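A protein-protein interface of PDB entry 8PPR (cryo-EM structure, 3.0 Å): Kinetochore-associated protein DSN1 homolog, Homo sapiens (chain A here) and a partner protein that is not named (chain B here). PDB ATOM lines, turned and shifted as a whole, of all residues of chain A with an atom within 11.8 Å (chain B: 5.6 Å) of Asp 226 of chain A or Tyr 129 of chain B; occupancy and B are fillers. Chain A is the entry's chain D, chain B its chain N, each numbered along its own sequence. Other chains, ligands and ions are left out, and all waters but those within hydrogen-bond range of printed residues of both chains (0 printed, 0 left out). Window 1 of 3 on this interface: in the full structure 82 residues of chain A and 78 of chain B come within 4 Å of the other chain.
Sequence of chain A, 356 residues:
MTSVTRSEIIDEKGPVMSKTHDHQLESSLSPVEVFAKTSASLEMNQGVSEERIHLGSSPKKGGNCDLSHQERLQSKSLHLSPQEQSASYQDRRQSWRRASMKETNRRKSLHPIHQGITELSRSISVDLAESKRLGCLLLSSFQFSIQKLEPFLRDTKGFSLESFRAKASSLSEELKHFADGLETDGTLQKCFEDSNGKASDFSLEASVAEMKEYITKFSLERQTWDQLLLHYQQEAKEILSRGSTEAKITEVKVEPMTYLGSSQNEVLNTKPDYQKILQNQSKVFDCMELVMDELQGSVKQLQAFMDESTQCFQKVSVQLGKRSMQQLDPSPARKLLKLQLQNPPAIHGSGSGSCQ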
ATOM      1  N   THR A 216      -7.930  -5.026  38.163  1.00  0.00           N
ATOM      2  CA  THR A 216      -9.067  -5.604  37.451  1.00  0.00           C
ATOM      3  C   THR A 216      -8.684  -5.985  36.025  1.00  0.00           C
ATOM      4  O   THR A 216      -9.006  -7.088  35.556  1.00  0.00           O
ATOM      5  CB  THR A 216     -10.239  -4.624  37.442  1.00  0.00           C
ATOM      6  OG1 THR A 216      -9.765  -3.314  37.109  1.00  0.00           O
ATOM      7  CG2 THR A 216     -10.910  -4.585  38.805  1.00  0.00           C
ATOM      8  N   LYS A 217      -7.981  -5.089  35.329  1.00  0.00           N
ATOM      9  CA  LYS A 217      -7.551  -5.382  33.966  1.00  0.00           C
ATOM     10  C   LYS A 217      -6.653  -6.609  33.930  1.00  0.00           C
ATOM     11  O   LYS A 217      -6.804  -7.480  33.065  1.00  0.00           O
ATOM     12  CB  LYS A 217      -6.824  -4.172  33.387  1.00  0.00           C
ATOM     13  CG  LYS A 217      -7.738  -3.080  32.869  1.00  0.00           C
ATOM     14  CD  LYS A 217      -6.947  -2.043  32.093  1.00  0.00           C
ATOM     15  CE  LYS A 217      -5.788  -1.513  32.924  1.00  0.00           C
ATOM     16  NZ  LYS A 217      -5.009  -0.470  32.205  1.00  0.00           N
ATOM     17  N   PHE A 218      -5.726  -6.706  34.881  1.00  0.00           N
ATOM     18  CA  PHE A 218      -4.786  -7.817  34.891  1.00  0.00           C
ATOM     19  C   PHE A 218      -5.461  -9.118  35.302  1.00  0.00           C
ATOM     20  O   PHE A 218      -5.066 -10.191  34.835  1.00  0.00           O
ATOM     21  CB  PHE A 218      -3.619  -7.485  35.818  1.00  0.00           C
ATOM     22  CG  PHE A 218      -2.815  -6.305  35.361  1.00  0.00           C
ATOM     23  CD1 PHE A 218      -2.780  -5.958  34.020  1.00  0.00           C
ATOM     24  CD2 PHE A 218      -2.125  -5.521  36.269  1.00  0.00           C
ATOM     25  CE1 PHE A 218      -2.053  -4.865  33.591  1.00  0.00           C
ATOM     26  CE2 PHE A 218      -1.401  -4.424  35.843  1.00  0.00           C
ATOM     27  CZ  PHE A 218      -1.363  -4.098  34.504  1.00  0.00           C
ATOM     28  N   SER A 219      -6.479  -9.045  36.163  1.00  0.00           N
ATOM     29  CA  SER A 219      -7.255 -10.235  36.496  1.00  0.00           C
ATOM     30  C   SER A 219      -8.004 -10.755  35.278  1.00  0.00           C
ATOM     31  O   SER A 219      -8.012 -11.962  35.012  1.00  0.00           O
ATOM     32  CB  SER A 219      -8.223  -9.925  37.637  1.00  0.00           C
ATOM     33  OG  SER A 219      -7.524  -9.623  38.831  1.00  0.00           O
ATOM     34  N   LEU A 220      -8.631  -9.855  34.516  1.00  0.00           N
ATOM     35  CA  LEU A 220      -9.253 -10.283  33.266  1.00  0.00           C
ATOM     36  C   LEU A 220      -8.218 -10.854  32.304  1.00  0.00           C
ATOM     37  O   LEU A 220      -8.486 -11.839  31.605  1.00  0.00           O
ATOM     38  CB  LEU A 220     -10.022  -9.130  32.619  1.00  0.00           C
ATOM     39  CG  LEU A 220     -11.452  -8.844  33.098  1.00  0.00           C
ATOM     40  CD1 LEU A 220     -12.342 -10.034  32.773  1.00  0.00           C
ATOM     41  CD2 LEU A 220     -11.540  -8.516  34.578  1.00  0.00           C
ATOM     42  N   GLU A 221      -7.026 -10.254  32.261  1.00  0.00           N
ATOM     43  CA  GLU A 221      -5.986 -10.749  31.363  1.00  0.00           C
ATOM     44  C   GLU A 221      -5.544 -12.160  31.735  1.00  0.00           C
ATOM     45  O   GLU A 221      -5.405 -13.021  30.860  1.00  0.00           O
ATOM     46  CB  GLU A 221      -4.792  -9.799  31.370  1.00  0.00           C
ATOM     47  CG  GLU A 221      -3.646 -10.256  30.484  1.00  0.00           C
ATOM     48  CD  GLU A 221      -2.749  -9.113  30.063  1.00  0.00           C
ATOM     49  OE1 GLU A 221      -3.215  -7.955  30.078  1.00  0.00           O
ATOM     50  OE2 GLU A 221      -1.577  -9.372  29.718  1.00  0.00           O
ATOM     51  N   ARG A 222      -5.315 -12.420  33.026  1.00  0.00           N
ATOM     52  CA  ARG A 222      -4.896 -13.758  33.429  1.00  0.00           C
ATOM     53  C   ARG A 222      -6.023 -14.767  33.254  1.00  0.00           C
ATOM     54  O   ARG A 222      -5.764 -15.929  32.919  1.00  0.00           O
ATOM     55  CB  ARG A 222      -4.406 -13.771  34.878  1.00  0.00           C
ATOM     56  CG  ARG A 222      -5.324 -13.098  35.865  1.00  0.00           C
ATOM     57  CD  ARG A 222      -4.973 -13.458  37.293  1.00  0.00           C
ATOM     58  NE  ARG A 222      -5.108 -14.887  37.542  1.00  0.00           N
ATOM     59  CZ  ARG A 222      -4.734 -15.488  38.663  1.00  0.00           C
ATOM     60  NH1 ARG A 222      -4.198 -14.810  39.665  1.00  0.00           N
ATOM     61  NH2 ARG A 222      -4.905 -16.801  38.783  1.00  0.00           N
ATOM     62  N   GLN A 223      -7.271 -14.347  33.472  1.00  0.00           N
ATOM     63  CA  GLN A 223      -8.398 -15.231  33.195  1.00  0.00           C
ATOM     64  C   GLN A 223      -8.441 -15.611  31.721  1.00  0.00           C
ATOM     65  O   GLN A 223      -8.634 -16.783  31.379  1.00  0.00           O
ATOM     66  CB  GLN A 223      -9.700 -14.554  33.615  1.00  0.00           C
ATOM     67  CG  GLN A 223      -9.917 -14.515  35.115  1.00  0.00           C
ATOM     68  CD  GLN A 223     -11.145 -13.718  35.499  1.00  0.00           C
ATOM     69  OE1 GLN A 223     -11.740 -13.034  34.666  1.00  0.00           O
ATOM     70  NE2 GLN A 223     -11.531 -13.797  36.766  1.00  0.00           N
ATOM     71  N   THR A 224      -8.251 -14.631  30.835  1.00  0.00           N
ATOM     72  CA  THR A 224      -8.228 -14.915  29.404  1.00  0.00           C
ATOM     73  C   THR A 224      -7.056 -15.818  29.042  1.00  0.00           C
ATOM     74  O   THR A 224      -7.186 -16.709  28.195  1.00  0.00           O
ATOM     75  CB  THR A 224      -8.164 -13.608  28.616  1.00  0.00           C
ATOM     76  OG1 THR A 224      -9.286 -12.787  28.959  1.00  0.00           O
ATOM     77  CG2 THR A 224      -8.188 -13.883  27.121  1.00  0.00           C
ATOM     78  N   TRP A 225      -5.902 -15.594  29.671  1.00  0.00           N
ATOM     79  CA  TRP A 225      -4.740 -16.446  29.437  1.00  0.00           C
ATOM     80  C   TRP A 225      -5.034 -17.890  29.819  1.00  0.00           C
ATOM     81  O   TRP A 225      -4.719 -18.825  29.070  1.00  0.00           O
ATOM     82  CB  TRP A 225      -3.551 -15.917  30.235  1.00  0.00           C
ATOM     83  CG  TRP A 225      -2.701 -14.949  29.495  1.00  0.00           C
ATOM     84  CD1 TRP A 225      -2.504 -13.633  29.795  1.00  0.00           C
ATOM     85  CD2 TRP A 225      -1.910 -15.220  28.335  1.00  0.00           C
ATOM     86  NE1 TRP A 225      -1.645 -13.065  28.886  1.00  0.00           N
ATOM     87  CE2 TRP A 225      -1.266 -14.020  27.978  1.00  0.00           C
ATOM     88  CE3 TRP A 225      -1.689 -16.362  27.558  1.00  0.00           C
ATOM     89  CZ2 TRP A 225      -0.415 -13.929  26.881  1.00  0.00           C
ATOM     90  CZ3 TRP A 225      -0.843 -16.269  26.471  1.00  0.00           C
ATOM     91  CH2 TRP A 225      -0.217 -15.062  26.142  1.00  0.00           C
ATOM     92  N   ASP A 226      -5.638 -18.088  30.989  1.00  0.00           N
ATOM     93  CA  ASP A 226      -5.979 -19.433  31.434  1.00  0.00           C
ATOM     94  C   ASP A 226      -7.007 -20.070  30.512  1.00  0.00           C
ATOM     95  O   ASP A 226      -6.918 -21.264  30.203  1.00  0.00           O
ATOM     96  CB  ASP A 226      -6.492 -19.388  32.872  1.00  0.00           C
ATOM     97  CG  ASP A 226      -5.408 -19.020  33.865  1.00  0.00           C
ATOM     98  OD1 ASP A 226      -4.236 -19.384  33.630  1.00  0.00           O
ATOM     99  OD2 ASP A 226      -5.724 -18.358  34.876  1.00  0.00           O
ATOM    100  N   GLN A 227      -7.992 -19.287  30.062  1.00  0.00           N
ATOM    101  CA  GLN A 227      -8.986 -19.807  29.130  1.00  0.00           C
ATOM    102  C   GLN A 227      -8.340 -20.244  27.824  1.00  0.00           C
ATOM    103  O   GLN A 227      -8.667 -21.307  27.286  1.00  0.00           O
ATOM    104  CB  GLN A 227     -10.067 -18.759  28.867  1.00  0.00           C
ATOM    105  CG  GLN A 227     -10.930 -18.443  30.073  1.00  0.00           C
ATOM    106  CD  GLN A 227     -11.558 -19.681  30.678  1.00  0.00           C
ATOM    107  OE1 GLN A 227     -11.998 -20.582  29.965  1.00  0.00           O
ATOM    108  NE2 GLN A 227     -11.599 -19.734  32.004  1.00  0.00           N
ATOM    109  N   LEU A 228      -7.420 -19.435  27.298  1.00  0.00           N
ATOM    110  CA  LEU A 228      -6.738 -19.797  26.061  1.00  0.00           C
ATOM    111  C   LEU A 228      -5.913 -21.063  26.242  1.00  0.00           C
ATOM    112  O   LEU A 228      -5.928 -21.954  25.383  1.00  0.00           O
ATOM    113  CB  LEU A 228      -5.853 -18.641  25.598  1.00  0.00           C
ATOM    114  CG  LEU A 228      -6.586 -17.477  24.933  1.00  0.00           C
ATOM    115  CD1 LEU A 228      -5.606 -16.562  24.217  1.00  0.00           C
ATOM    116  CD2 LEU A 228      -7.651 -17.987  23.976  1.00  0.00           C
ATOM    117  N   LEU A 229      -5.189 -21.160  27.360  1.00  0.00           N
ATOM    118  CA  LEU A 229      -4.382 -22.348  27.614  1.00  0.00           C
ATOM    119  C   LEU A 229      -5.247 -23.596  27.704  1.00  0.00           C
ATOM    120  O   LEU A 229      -4.932 -24.624  27.091  1.00  0.00           O
ATOM    121  CB  LEU A 229      -3.569 -22.167  28.894  1.00  0.00           C
ATOM    122  CG  LEU A 229      -2.520 -23.244  29.178  1.00  0.00           C
ATOM    123  CD1 LEU A 229      -1.234 -22.617  29.681  1.00  0.00           C
ATOM    124  CD2 LEU A 229      -3.045 -24.260  30.186  1.00  0.00           C
ATOM    125  N   LEU A 230      -6.342 -23.528  28.467  1.00  0.00           N
ATOM    126  CA  LEU A 230      -7.203 -24.696  28.608  1.00  0.00           C
ATOM    127  C   LEU A 230      -7.857 -25.054  27.282  1.00  0.00           C
ATOM    128  O   LEU A 230      -7.972 -26.234  26.941  1.00  0.00           O
ATOM    129  CB  LEU A 230      -8.251 -24.465  29.700  1.00  0.00           C
ATOM    130  CG  LEU A 230      -9.315 -23.368  29.600  1.00  0.00           C
ATOM    131  CD1 LEU A 230     -10.550 -23.829  28.835  1.00  0.00           C
ATOM    132  CD2 LEU A 230      -9.698 -22.881  30.990  1.00  0.00           C
ATOM    133  N   HIS A 231      -8.271 -24.047  26.510  1.00  0.00           N
ATOM    134  CA  HIS A 231      -8.860 -24.304  25.203  1.00  0.00           C
ATOM    135  C   HIS A 231      -7.884 -25.038  24.298  1.00  0.00           C
ATOM    136  O   HIS A 231      -8.236 -26.041  23.668  1.00  0.00           O
ATOM    137  CB  HIS A 231      -9.293 -22.986  24.564  1.00  0.00           C
ATOM    138  CG  HIS A 231      -9.972 -23.151  23.242  1.00  0.00           C
ATOM    139  ND1 HIS A 231      -9.964 -22.169  22.275  1.00  0.00           N
ATOM    140  CD2 HIS A 231     -10.672 -24.187  22.722  1.00  0.00           C
ATOM    141  CE1 HIS A 231     -10.635 -22.590  21.218  1.00  0.00           C
ATOM    142  NE2 HIS A 231     -11.075 -23.811  21.462  1.00  0.00           N
ATOM    143  N   TYR A 232      -6.648 -24.553  24.224  1.00  0.00           N
ATOM    144  CA  TYR A 232      -5.689 -25.160  23.309  1.00  0.00           C
ATOM    145  C   TYR A 232      -5.285 -26.555  23.766  1.00  0.00           C
ATOM    146  O   TYR A 232      -5.186 -27.475  22.945  1.00  0.00           O
ATOM    147  CB  TYR A 232      -4.481 -24.244  23.153  1.00  0.00           C
ATOM    148  CG  TYR A 232      -4.838 -22.973  22.423  1.00  0.00           C
ATOM    149  CD1 TYR A 232      -6.032 -22.871  21.719  1.00  0.00           C
ATOM    150  CD2 TYR A 232      -3.999 -21.872  22.450  1.00  0.00           C
ATOM    151  CE1 TYR A 232      -6.373 -21.715  21.054  1.00  0.00           C
ATOM    152  CE2 TYR A 232      -4.332 -20.709  21.785  1.00  0.00           C
ATOM    153  CZ  TYR A 232      -5.521 -20.635  21.089  1.00  0.00           C
ATOM    154  OH  TYR A 232      -5.855 -19.478  20.427  1.00  0.00           O
ATOM    155  N   GLN A 233      -5.061 -26.741  25.069  1.00  0.00           N
ATOM    156  CA  GLN A 233      -4.699 -28.069  25.551  1.00  0.00           C
ATOM    157  C   GLN A 233      -5.847 -29.055  25.369  1.00  0.00           C
ATOM    158  O   GLN A 233      -5.621 -30.212  24.990  1.00  0.00           O
ATOM    159  CB  GLN A 233      -4.248 -28.000  27.013  1.00  0.00           C
ATOM    160  CG  GLN A 233      -5.345 -27.715  28.021  1.00  0.00           C
ATOM    161  CD  GLN A 233      -4.821 -27.605  29.438  1.00  0.00           C
ATOM    162  OE1 GLN A 233      -3.662 -27.920  29.710  1.00  0.00           O
ATOM    163  NE2 GLN A 233      -5.672 -27.156  30.352  1.00  0.00           N
ATOM    164  N   GLN A 234      -7.088 -28.616  25.605  1.00  0.00           N
ATOM    165  CA  GLN A 234      -8.230 -29.501  25.420  1.00  0.00           C
ATOM    166  C   GLN A 234      -8.426 -29.834  23.948  1.00  0.00           C
ATOM    167  O   GLN A 234      -8.759 -30.973  23.606  1.00  0.00           O
ATOM    168  CB  GLN A 234      -9.489 -28.875  26.028  1.00  0.00           C
ATOM    169  CG  GLN A 234     -10.242 -27.907  25.128  1.00  0.00           C
ATOM    170  CD  GLN A 234     -11.592 -27.515  25.687  1.00  0.00           C
ATOM    171  OE1 GLN A 234     -11.867 -27.708  26.870  1.00  0.00           O
ATOM    172  NE2 GLN A 234     -12.444 -26.956  24.835  1.00  0.00           N
ATOM    173  N   GLU A 235      -8.194 -28.865  23.059  1.00  0.00           N
ATOM    174  CA  GLU A 235      -8.275 -29.143  21.631  1.00  0.00           C
ATOM    175  C   GLU A 235      -7.220 -30.155  21.213  1.00  0.00           C
ATOM    176  O   GLU A 235      -7.510 -31.094  20.461  1.00  0.00           O
ATOM    177  CB  GLU A 235      -8.117 -27.846  20.844  1.00  0.00           C
ATOM    178  CG  GLU A 235      -8.123 -28.029  19.342  1.00  0.00           C
ATOM    179  CD  GLU A 235      -8.236 -26.712  18.606  1.00  0.00           C
ATOM    180  OE1 GLU A 235      -8.272 -25.659  19.276  1.00  0.00           O
ATOM    181  OE2 GLU A 235      -8.289 -26.731  17.359  1.00  0.00           O
ATOM    182  N   LYS A 237      -5.662 -32.453  23.094  1.00  0.00           N
ATOM    183  CA  LYS A 237      -5.925 -33.787  23.625  1.00  0.00           C
ATOM    184  C   LYS A 237      -7.144 -34.414  22.960  1.00  0.00           C
ATOM    185  O   LYS A 237      -7.172 -35.626  22.731  1.00  0.00           O
ATOM    186  CB  LYS A 237      -6.100 -33.745  25.143  1.00  0.00           C
ATOM    187  CG  LYS A 237      -7.200 -32.835  25.635  1.00  0.00           C
ATOM    188  CD  LYS A 237      -7.374 -32.942  27.138  1.00  0.00           C
ATOM    189  CE  LYS A 237      -6.110 -32.522  27.867  1.00  0.00           C
ATOM    190  NZ  LYS A 237      -6.315 -32.458  29.339  1.00  0.00           N
ATOM    191  N   THR B 124       4.753 -13.602  34.716  1.00  0.00           N
ATOM    192  CA  THR B 124       5.096 -15.011  34.557  1.00  0.00           C
ATOM    193  C   THR B 124       4.196 -15.683  33.531  1.00  0.00           C
ATOM    194  O   THR B 124       4.659 -16.505  32.733  1.00  0.00           O
ATOM    195  CB  THR B 124       5.003 -15.732  35.900  1.00  0.00           C
ATOM    196  OG1 THR B 124       3.693 -15.548  36.454  1.00  0.00           O
ATOM    197  CG2 THR B 124       6.046 -15.197  36.869  1.00  0.00           C
ATOM    198  N   LYS B 125       2.904 -15.352  33.542  1.00  0.00           N
ATOM    199  CA  LYS B 125       1.986 -15.918  32.561  1.00  0.00           C
ATOM    200  C   LYS B 125       2.387 -15.521  31.147  1.00  0.00           C
ATOM    201  O   LYS B 125       2.432 -16.366  30.246  1.00  0.00           O
ATOM    202  CB  LYS B 125       0.559 -15.466  32.863  1.00  0.00           C
ATOM    203  CG  LYS B 125      -0.069 -16.174  34.049  1.00  0.00           C
ATOM    204  CD  LYS B 125      -1.540 -15.824  34.183  1.00  0.00           C
ATOM    205  CE  LYS B 125      -2.140 -16.444  35.433  1.00  0.00           C
ATOM    206  NZ  LYS B 125      -1.799 -17.887  35.556  1.00  0.00           N
ATOM    207  N   ARG B 126       2.712 -14.243  30.946  1.00  0.00           N
ATOM    208  CA  ARG B 126       3.145 -13.781  29.632  1.00  0.00           C
ATOM    209  C   ARG B 126       4.410 -14.499  29.189  1.00  0.00           C
ATOM    210  O   ARG B 126       4.560 -14.842  28.011  1.00  0.00           O
ATOM    211  CB  ARG B 126       3.379 -12.273  29.657  1.00  0.00           C
ATOM    212  CG  ARG B 126       2.149 -11.438  29.370  1.00  0.00           C
ATOM    213  CD  ARG B 126       2.444  -9.970  29.610  1.00  0.00           C
ATOM    214  NE  ARG B 126       1.230  -9.173  29.723  1.00  0.00           N
ATOM    215  CZ  ARG B 126       1.196  -7.928  30.176  1.00  0.00           C
ATOM    216  NH1 ARG B 126       2.296  -7.305  30.565  1.00  0.00           N
ATOM    217  NH2 ARG B 126       0.030  -7.292  30.241  1.00  0.00           N
ATOM    218  N   LYS B 127       5.339 -14.724  30.117  1.00  0.00           N
ATOM    219  CA  LYS B 127       6.585 -15.387  29.748  1.00  0.00           C
ATOM    220  C   LYS B 127       6.366 -16.862  29.429  1.00  0.00           C
ATOM    221  O   LYS B 127       7.000 -17.405  28.517  1.00  0.00           O
ATOM    222  CB  LYS B 127       7.615 -15.231  30.864  1.00  0.00           C
ATOM    223  CG  LYS B 127       9.038 -15.525  30.425  1.00  0.00           C
ATOM    224  CD  LYS B 127       9.924 -15.853  31.612  1.00  0.00           C
ATOM    225  CE  LYS B 127      10.098 -14.646  32.515  1.00  0.00           C
ATOM    226  NZ  LYS B 127      10.987 -13.618  31.905  1.00  0.00           N
ATOM    227  N   GLN B 128       5.471 -17.527  30.160  1.00  0.00           N
ATOM    228  CA  GLN B 128       5.393 -18.982  30.110  1.00  0.00           C
ATOM    229  C   GLN B 128       4.354 -19.503  29.122  1.00  0.00           C
ATOM    230  O   GLN B 128       4.656 -20.400  28.328  1.00  0.00           O
ATOM    231  CB  GLN B 128       5.103 -19.536  31.507  1.00  0.00           C
ATOM    232  CG  GLN B 128       6.204 -19.274  32.522  1.00  0.00           C
ATOM    233  CD  GLN B 128       7.509 -19.963  32.164  1.00  0.00           C
ATOM    234  OE1 GLN B 128       7.534 -20.904  31.370  1.00  0.00           O
ATOM    235  NE2 GLN B 128       8.603 -19.492  32.750  1.00  0.00           N
ATOM    236  N   TYR B 129       3.134 -18.967  29.164  1.00  0.00           N
ATOM    237  CA  TYR B 129       2.042 -19.551  28.386  1.00  0.00           C
ATOM    238  C   TYR B 129       2.337 -19.704  26.898  1.00  0.00           C
ATOM    239  O   TYR B 129       2.000 -20.768  26.348  1.00  0.00           O
ATOM    240  CB  TYR B 129       0.763 -18.733  28.592  1.00  0.00           C
ATOM    241  CG  TYR B 129       0.155 -18.889  29.962  1.00  0.00           C
ATOM    242  CD1 TYR B 129       0.587 -19.887  30.824  1.00  0.00           C
ATOM    243  CD2 TYR B 129      -0.868 -18.058  30.385  1.00  0.00           C
ATOM    244  CE1 TYR B 129       0.027 -20.039  32.076  1.00  0.00           C
ATOM    245  CE2 TYR B 129      -1.435 -18.205  31.631  1.00  0.00           C
ATOM    246  CZ  TYR B 129      -0.985 -19.194  32.474  1.00  0.00           C
ATOM    247  OH  TYR B 129      -1.551 -19.337  33.719  1.00  0.00           O
ATOM    248  N   PRO B 130       2.938 -18.734  26.198  1.00  0.00           N
ATOM    249  CA  PRO B 130       3.138 -18.908  24.749  1.00  0.00           C
ATOM    250  C   PRO B 130       3.898 -20.166  24.375  1.00  0.00           C
ATOM    251  O   PRO B 130       3.610 -20.756  23.330  1.00  0.00           O
ATOM    252  CB  PRO B 130       3.914 -17.646  24.353  1.00  0.00           C
ATOM    253  CG  PRO B 130       3.500 -16.636  25.347  1.00  0.00           C
ATOM    254  CD  PRO B 130       3.334 -17.382  26.634  1.00  0.00           C
ATOM    255  N   ARG B 131       4.857 -20.600  25.193  1.00  0.00           N
ATOM    256  CA  ARG B 131       5.599 -21.817  24.878  1.00  0.00           C
ATOM    257  C   ARG B 131       4.683 -23.037  24.866  1.00  0.00           C
ATOM    258  O   ARG B 131       4.704 -23.839  23.923  1.00  0.00           O
ATOM    259  CB  ARG B 131       6.733 -22.000  25.883  1.00  0.00           C
ATOM    260  CG  ARG B 131       7.673 -23.147  25.570  1.00  0.00           C
ATOM    261  CD  ARG B 131       8.786 -23.200  26.596  1.00  0.00           C
ATOM    262  NE  ARG B 131       8.272 -23.544  27.916  1.00  0.00           N
ATOM    263  CZ  ARG B 131       8.263 -22.720  28.954  1.00  0.00           C
ATOM    264  NH1 ARG B 131       8.731 -21.486  28.861  1.00  0.00           N
ATOM    265  NH2 ARG B 131       7.768 -23.142  30.114  1.00  0.00           N
ATOM    266  N   LYS B 132       3.869 -23.190  25.913  1.00  0.00           N
ATOM    267  CA  LYS B 132       2.939 -24.313  25.973  1.00  0.00           C
ATOM    268  C   LYS B 132       1.899 -24.215  24.866  1.00  0.00           C
ATOM    269  O   LYS B 132       1.516 -25.230  24.268  1.00  0.00           O
ATOM    270  CB  LYS B 132       2.265 -24.360  27.343  1.00  0.00           C
ATOM    271  CG  LYS B 132       3.209 -24.531  28.542  1.00  0.00           C
ATOM    272  CD  LYS B 132       3.839 -25.920  28.634  1.00  0.00           C
ATOM    273  CE  LYS B 132       5.204 -25.982  27.960  1.00  0.00           C
ATOM    274  NZ  LYS B 132       5.855 -27.308  28.149  1.00  0.00           N
ATOM    275  N   ILE B 133       1.429 -22.998  24.586  1.00  0.00           N
ATOM    276  CA  ILE B 133       0.505 -22.785  23.479  1.00  0.00           C
ATOM    277  C   ILE B 133       1.117 -23.274  22.177  1.00  0.00           C
ATOM    278  O   ILE B 133       0.472 -23.980  21.393  1.00  0.00           O
ATOM    279  CB  ILE B 133       0.122 -21.295  23.391  1.00  0.00           C
ATOM    280  CG1 ILE B 133      -0.603 -20.843  24.662  1.00  0.00           C
ATOM    281  CG2 ILE B 133      -0.694 -21.025  22.141  1.00  0.00           C
ATOM    282  CD1 ILE B 133      -1.664 -21.810  25.141  1.00  0.00           C
ATOM    283  N   LEU B 134       2.377 -22.918  21.936  1.00  0.00           N
ATOM    284  CA  LEU B 134       3.040 -23.304  20.699  1.00  0.00           C
ATOM    285  C   LEU B 134       3.222 -24.813  20.626  1.00  0.00           C
ATOM    286  O   LEU B 134       3.077 -25.412  19.555  1.00  0.00           O
ATOM    287  CB  LEU B 134       4.381 -22.586  20.595  1.00  0.00           C
ATOM    288  CG  LEU B 134       4.952 -22.455  19.189  1.00  0.00           C
ATOM    289  CD1 LEU B 134       3.893 -21.860  18.273  1.00  0.00           C
ATOM    290  CD2 LEU B 134       6.202 -21.594  19.208  1.00  0.00           C
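OH of Tyr 129 of chain B lies within hydrogen-bond range of OD1 of Asp 226 of chain A (2.7 Å).
The side-chain carboxylate (OE2) of Glu 221 of chain A is in salt-bridge range of the guanidinium group (NH2) of Arg 126 of chain B, 2.7 Å away.
NZ of Lys 125 of chain B lies within salt-bridge range of OD1 of Asp 226 of chain A.
Among the printed residues, merely in contact across the chains: Trp 225 of chain A with Tyr 129 of chain B, Tyr 232 of chain A with Ile 133 of chain B, Leu 229 of chain A with Tyr 129 of chain B, Arg 222 of chain A with Lys 125 of chain B and Leu 229 of chain A with Ile 133 of chain B.
Among the printed residues, 8 pairs touch across the chains.
Among the printed residues, Asp or Glu carboxylates within 4 Å of a Lys or Arg side-chain nitrogen of the other chain: Glu 221 of chain A with Arg 126 of chain B and Asp 226 of chain A with Lys 125 of chain B.
Asp 226 of chain A touches just these residues of chain B: Lys 125 (3.4 Å) and Tyr 129 (2.7 Å).
Of chain A, only Arg 222 (3.5 Å) and Asp 226 (3.4 Å) come within 4 Å of Lys 125 of chain B.
No residue of chain A comes within 4 Å of Pro 130 of chain B.
No residue of chain A comes within 4 Å of Arg 131 of chain B.
Of chain A, only Leu 229 (3.7 Å) and Tyr 232 (3.4 Å) come within 4 Å of Ile 133 of chain B.
Of the printed residues of chain B, Arg 222 of chain A touches Lys 125 (3.5 Å).
Printed residues of chain A within 4 Å of Arg 126 of chain B: Glu 221.
Lys 237 of chain A touches none of the printed residues of chain B.
Lys 127 of chain B touches none of the printed residues of chain A.
The nearest printed residue of chain B that does not touch Asp 226 of chain A is Ile 133 of chain B (7.3 Å).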
